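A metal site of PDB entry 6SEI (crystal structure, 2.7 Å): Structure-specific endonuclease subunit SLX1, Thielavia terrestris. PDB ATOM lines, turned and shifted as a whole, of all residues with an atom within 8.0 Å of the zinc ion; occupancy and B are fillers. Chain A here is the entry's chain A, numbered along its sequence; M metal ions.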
ATOM      1  N   LYS A 216      23.346  15.673 -12.004  1.00  0.00           N
ATOM      2  CA  LYS A 216      22.680  16.224 -10.838  1.00  0.00           C
ATOM      3  C   LYS A 216      21.369  15.503 -10.551  1.00  0.00           C
ATOM      4  O   LYS A 216      21.008  15.275  -9.388  1.00  0.00           O
ATOM      5  CB  LYS A 216      22.430  17.722 -11.024  1.00  0.00           C
ATOM      6  CG  LYS A 216      21.843  18.427  -9.822  1.00  0.00           C
ATOM      7  CD  LYS A 216      21.554  19.894 -10.116  1.00  0.00           C
ATOM      8  CE  LYS A 216      20.268  20.060 -10.921  1.00  0.00           C
ATOM      9  NZ  LYS A 216      20.135  21.441 -11.471  1.00  0.00           N
ATOM     10  N   VAL A 230       8.440  22.264  -5.293  1.00  0.00           N
ATOM     11  CA  VAL A 230       8.686  23.674  -5.060  1.00  0.00           C
ATOM     12  C   VAL A 230       7.467  24.534  -5.329  1.00  0.00           C
ATOM     13  O   VAL A 230       7.443  25.702  -4.929  1.00  0.00           O
ATOM     14  CB  VAL A 230       9.877  24.185  -5.897  1.00  0.00           C
ATOM     15  CG1 VAL A 230      11.186  23.648  -5.353  1.00  0.00           C
ATOM     16  CG2 VAL A 230       9.698  23.791  -7.354  1.00  0.00           C
ATOM     17  N   LEU A 245      12.978  18.635 -12.788  1.00  0.00           N
ATOM     18  CA  LEU A 245      14.090  19.181 -12.032  1.00  0.00           C
ATOM     19  C   LEU A 245      14.543  20.504 -12.648  1.00  0.00           C
ATOM     20  O   LEU A 245      14.637  20.635 -13.870  1.00  0.00           O
ATOM     21  CB  LEU A 245      15.257  18.189 -12.015  1.00  0.00           C
ATOM     22  CG  LEU A 245      16.555  18.597 -11.345  1.00  0.00           C
ATOM     23  CD1 LEU A 245      16.331  18.915  -9.879  1.00  0.00           C
ATOM     24  CD2 LEU A 245      17.577  17.490 -11.528  1.00  0.00           C
ATOM     25  N   CYS A 246      14.824  21.482 -11.778  1.00  0.00           N
ATOM     26  CA  CYS A 246      15.317  22.767 -12.260  1.00  0.00           C
ATOM     27  C   CYS A 246      16.627  22.579 -13.020  1.00  0.00           C
ATOM     28  O   CYS A 246      17.500  21.808 -12.619  1.00  0.00           O
ATOM     29  CB  CYS A 246      15.526  23.734 -11.094  1.00  0.00           C
ATOM     30  SG  CYS A 246      16.569  25.165 -11.470  1.00  0.00           S
ATOM     31  N   THR A 247      16.763  23.311 -14.132  1.00  0.00           N
ATOM     32  CA  THR A 247      17.891  23.120 -15.036  1.00  0.00           C
ATOM     33  C   THR A 247      19.159  23.837 -14.592  1.00  0.00           C
ATOM     34  O   THR A 247      20.231  23.545 -15.140  1.00  0.00           O
ATOM     35  CB  THR A 247      17.518  23.592 -16.447  1.00  0.00           C
ATOM     36  OG1 THR A 247      17.071  24.951 -16.396  1.00  0.00           O
ATOM     37  CG2 THR A 247      16.388  22.740 -17.019  1.00  0.00           C
ATOM     38  N   ASN A 248      19.074  24.747 -13.639  1.00  0.00           N
ATOM     39  CA  ASN A 248      20.221  25.548 -13.252  1.00  0.00           C
ATOM     40  C   ASN A 248      21.185  24.747 -12.381  1.00  0.00           C
ATOM     41  O   ASN A 248      20.767  23.958 -11.538  1.00  0.00           O
ATOM     42  CB  ASN A 248      19.771  26.803 -12.513  1.00  0.00           C
ATOM     43  CG  ASN A 248      19.227  27.865 -13.442  1.00  0.00           C
ATOM     44  OD1 ASN A 248      18.051  28.228 -13.379  1.00  0.00           O
ATOM     45  ND2 ASN A 248      20.082  28.361 -14.330  1.00  0.00           N
ATOM     46  N   GLN A 249      22.477  24.951 -12.608  1.00  0.00           N
ATOM     47  CA  GLN A 249      23.505  24.177 -11.915  1.00  0.00           C
ATOM     48  C   GLN A 249      23.438  24.422 -10.412  1.00  0.00           C
ATOM     49  O   GLN A 249      23.259  25.551  -9.953  1.00  0.00           O
ATOM     50  CB  GLN A 249      24.890  24.531 -12.458  1.00  0.00           C
ATOM     51  CG  GLN A 249      25.364  25.945 -12.134  1.00  0.00           C
ATOM     52  CD  GLN A 249      26.814  25.988 -11.682  1.00  0.00           C
ATOM     53  OE1 GLN A 249      27.711  25.544 -12.399  1.00  0.00           O
ATOM     54  NE2 GLN A 249      27.059  26.542 -10.495  1.00  0.00           N
ATOM     55  N   GLY A 250      23.564  23.338  -9.644  1.00  0.00           N
ATOM     56  CA  GLY A 250      23.626  23.413  -8.200  1.00  0.00           C
ATOM     57  C   GLY A 250      22.317  23.655  -7.484  1.00  0.00           C
ATOM     58  O   GLY A 250      22.320  23.737  -6.257  1.00  0.00           O
ATOM     59  N   CYS A 251      21.207  23.765  -8.210  1.00  0.00           N
ATOM     60  CA  CYS A 251      19.911  24.002  -7.600  1.00  0.00           C
ATOM     61  C   CYS A 251      19.099  22.719  -7.517  1.00  0.00           C
ATOM     62  O   CYS A 251      19.083  21.910  -8.462  1.00  0.00           O
ATOM     63  CB  CYS A 251      19.113  25.050  -8.376  1.00  0.00           C
ATOM     64  SG  CYS A 251      17.399  25.167  -7.825  1.00  0.00           S
ATOM     65  N   ASP A 252      18.361  22.573  -6.411  1.00  0.00           N
ATOM     66  CA  ASP A 252      17.679  21.340  -6.039  1.00  0.00           C
ATOM     67  C   ASP A 252      16.274  21.211  -6.595  1.00  0.00           C
ATOM     68  O   ASP A 252      15.760  20.083  -6.660  1.00  0.00           O
ATOM     69  CB  ASP A 252      17.569  21.233  -4.520  1.00  0.00           C
ATOM     70  CG  ASP A 252      18.777  20.588  -3.899  1.00  0.00           C
ATOM     71  OD1 ASP A 252      19.639  20.127  -4.660  1.00  0.00           O
ATOM     72  OD2 ASP A 252      18.861  20.560  -2.658  1.00  0.00           O
ATOM     73  N   GLY A 253      15.640  22.309  -6.970  1.00  0.00           N
ATOM     74  CA  GLY A 253      14.208  22.352  -7.261  1.00  0.00           C
ATOM     75  C   GLY A 253      13.623  21.204  -8.067  1.00  0.00           C
ATOM     76  O   GLY A 253      13.875  21.093  -9.267  1.00  0.00           O
ATOM     77  N   VAL A 254      12.849  20.352  -7.399  1.00  0.00           N
ATOM     78  CA  VAL A 254      12.066  19.308  -8.051  1.00  0.00           C
ATOM     79  C   VAL A 254      10.587  19.615  -7.842  1.00  0.00           C
ATOM     80  O   VAL A 254      10.181  20.086  -6.776  1.00  0.00           O
ATOM     81  CB  VAL A 254      12.395  17.897  -7.509  1.00  0.00           C
ATOM     82  CG1 VAL A 254      11.848  16.833  -8.447  1.00  0.00           C
ATOM     83  CG2 VAL A 254      13.894  17.730  -7.335  1.00  0.00           C
ATOM     84  N   TRP A 260       4.959  22.455 -12.332  1.00  0.00           N
ATOM     85  CA  TRP A 260       5.899  23.316 -13.039  1.00  0.00           C
ATOM     86  C   TRP A 260       5.207  24.089 -14.147  1.00  0.00           C
ATOM     87  O   TRP A 260       5.307  25.314 -14.233  1.00  0.00           O
ATOM     88  CB  TRP A 260       7.045  22.486 -13.628  1.00  0.00           C
ATOM     89  CG  TRP A 260       8.213  22.250 -12.710  1.00  0.00           C
ATOM     90  CD1 TRP A 260       8.701  21.046 -12.313  1.00  0.00           C
ATOM     91  CD2 TRP A 260       9.088  23.241 -12.132  1.00  0.00           C
ATOM     92  NE1 TRP A 260       9.791  21.207 -11.504  1.00  0.00           N
ATOM     93  CE2 TRP A 260      10.053  22.537 -11.378  1.00  0.00           C
ATOM     94  CE3 TRP A 260       9.138  24.633 -12.172  1.00  0.00           C
ATOM     95  CZ2 TRP A 260      11.058  23.195 -10.667  1.00  0.00           C
ATOM     96  CZ3 TRP A 260      10.126  25.277 -11.468  1.00  0.00           C
ATOM     97  CH2 TRP A 260      11.075  24.558 -10.720  1.00  0.00           C
ATOM     98  N   GLN A 279      10.667  30.550 -14.545  1.00  0.00           N
ATOM     99  CA  GLN A 279      11.583  30.904 -13.471  1.00  0.00           C
ATOM    100  C   GLN A 279      11.387  29.940 -12.321  1.00  0.00           C
ATOM    101  O   GLN A 279      10.246  29.654 -11.933  1.00  0.00           O
ATOM    102  CB  GLN A 279      11.348  32.354 -13.012  1.00  0.00           C
ATOM    103  CG  GLN A 279      12.513  32.974 -12.255  1.00  0.00           C
ATOM    104  CD  GLN A 279      12.069  34.000 -11.226  1.00  0.00           C
ATOM    105  OE1 GLN A 279      12.640  34.077 -10.132  1.00  0.00           O
ATOM    106  NE2 GLN A 279      11.067  34.799 -11.574  1.00  0.00           N
ATOM    107  N   CYS A 280      12.490  29.427 -11.776  1.00  0.00           N
ATOM    108  CA  CYS A 280      12.442  28.484 -10.662  1.00  0.00           C
ATOM    109  C   CYS A 280      12.055  29.200  -9.375  1.00  0.00           C
ATOM    110  O   CYS A 280      12.687  30.207  -9.031  1.00  0.00           O
ATOM    111  CB  CYS A 280      13.794  27.804 -10.494  1.00  0.00           C
ATOM    112  SG  CYS A 280      13.962  26.829  -8.989  1.00  0.00           S
ATOM    113  N   PRO A 281      11.052  28.715  -8.635  1.00  0.00           N
ATOM    114  CA  PRO A 281      10.672  29.387  -7.390  1.00  0.00           C
ATOM    115  C   PRO A 281      11.707  29.252  -6.273  1.00  0.00           C
ATOM    116  O   PRO A 281      11.611  29.994  -5.279  1.00  0.00           O
ATOM    117  CB  PRO A 281       9.353  28.692  -6.992  1.00  0.00           C
ATOM    118  CG  PRO A 281       8.916  27.937  -8.219  1.00  0.00           C
ATOM    119  CD  PRO A 281      10.185  27.566  -8.926  1.00  0.00           C
ATOM    120  N   LYS A 282      12.691  28.364  -6.402  1.00  0.00           N
ATOM    121  CA  LYS A 282      13.680  28.145  -5.356  1.00  0.00           C
ATOM    122  C   LYS A 282      14.931  28.981  -5.582  1.00  0.00           C
ATOM    123  O   LYS A 282      15.352  29.741  -4.697  1.00  0.00           O
ATOM    124  CB  LYS A 282      14.046  26.659  -5.274  1.00  0.00           C
ATOM    125  CG  LYS A 282      15.237  26.369  -4.387  1.00  0.00           C
ATOM    126  CD  LYS A 282      15.539  24.887  -4.313  1.00  0.00           C
ATOM    127  CE  LYS A 282      15.006  24.268  -3.042  1.00  0.00           C
ATOM    128  NZ  LYS A 282      15.823  23.108  -2.593  1.00  0.00           N
ATOM    129  N   CYS A 283      15.561  28.846  -6.756  1.00  0.00           N
ATOM    130  CA  CYS A 283      16.793  29.568  -7.066  1.00  0.00           C
ATOM    131  C   CYS A 283      16.556  30.825  -7.882  1.00  0.00           C
ATOM    132  O   CYS A 283      17.502  31.610  -8.057  1.00  0.00           O
ATOM    133  CB  CYS A 283      17.774  28.653  -7.798  1.00  0.00           C
ATOM    134  SG  CYS A 283      17.353  28.295  -9.520  1.00  0.00           S
ATOM    135  N   GLY A 284      15.346  31.040  -8.391  1.00  0.00           N
ATOM    136  CA  GLY A 284      15.064  32.222  -9.179  1.00  0.00           C
ATOM    137  C   GLY A 284      15.688  32.239 -10.557  1.00  0.00           C
ATOM    138  O   GLY A 284      15.642  33.280 -11.229  1.00  0.00           O
ATOM    139  N   GLY A 285      16.271  31.128 -10.994  1.00  0.00           N
ATOM    140  CA  GLY A 285      16.930  31.094 -12.288  1.00  0.00           C
ATOM    141  C   GLY A 285      15.951  30.836 -13.415  1.00  0.00           C
ATOM    142  O   GLY A 285      14.996  30.065 -13.279  1.00  0.00           O
ATOM    143  N   GLU A 286      16.180  31.507 -14.542  1.00  0.00           N
ATOM    144  CA  GLU A 286      15.340  31.334 -15.716  1.00  0.00           C
ATOM    145  C   GLU A 286      15.569  29.968 -16.340  1.00  0.00           C
ATOM    146  O   GLU A 286      16.701  29.468 -16.393  1.00  0.00           O
ATOM    147  CB  GLU A 286      15.611  32.439 -16.736  1.00  0.00           C
ATOM    148  CG  GLU A 286      14.898  33.752 -16.449  1.00  0.00           C
ATOM    149  CD  GLU A 286      13.463  33.776 -16.975  1.00  0.00           C
ATOM    150  OE1 GLU A 286      12.626  34.492 -16.382  1.00  0.00           O
ATOM    151  OE2 GLU A 286      13.172  33.089 -17.979  1.00  0.00           O
ATOM    152  N   MET A 287      14.491  29.375 -16.840  1.00  0.00           N
ATOM    153  CA  MET A 287      14.528  28.040 -17.420  1.00  0.00           C
ATOM    154  C   MET A 287      13.777  28.011 -18.751  1.00  0.00           C
ATOM    155  O   MET A 287      12.832  28.773 -18.964  1.00  0.00           O
ATOM    156  CB  MET A 287      13.887  26.994 -16.518  1.00  0.00           C
ATOM    157  CG  MET A 287      14.692  26.585 -15.318  1.00  0.00           C
ATOM    158  SD  MET A 287      13.701  25.392 -14.426  1.00  0.00           S
ATOM    159  CE  MET A 287      12.514  26.488 -13.669  1.00  0.00           C
HETATM  160 ZN    ZN M   1      16.183  26.237  -9.490  1.00  0.00          ZN
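N of Cys 246 lies within hydrogen-bond range of O of Gly 253 (2.7 Å). The side-chain sulfur (SG) of Cys 246 lies close to the backbone NH (N) of Asn 248 (3.3 Å). The backbone carbonyl oxygen of Cys 246 sits at hydrogen-bond distance from the side-chain amino group of Lys 216 (2.9 Å). N of Gly 253 lies close to SG of Cys 251, at 3.5 Å. O of Cys 251 lies within hydrogen-bond range of NZ of Lys 216 (3.2 Å). N of Lys 282 sits close to SG of Cys 280. The backbone carbonyl oxygen (O) of Gly 285 sits at hydrogen-bond distance from the backbone NH (N) of Cys 280 (3.0 Å). The side-chain sulfur of Cys 283 lies close to the backbone NH of Gly 285.
Within 4 Å of the zinc ion: Cys 246, Cys 251, Cys 280 and Cys 283. The nearest printed residue that does not touch the zinc ion is Gly 253 (4.7 Å).
The zinc ion is bound by SG of Cys 246, SG of Cys 251, SG of Cys 280 and SG of Cys 283. The zinc ion has four donor atoms within binding distance.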
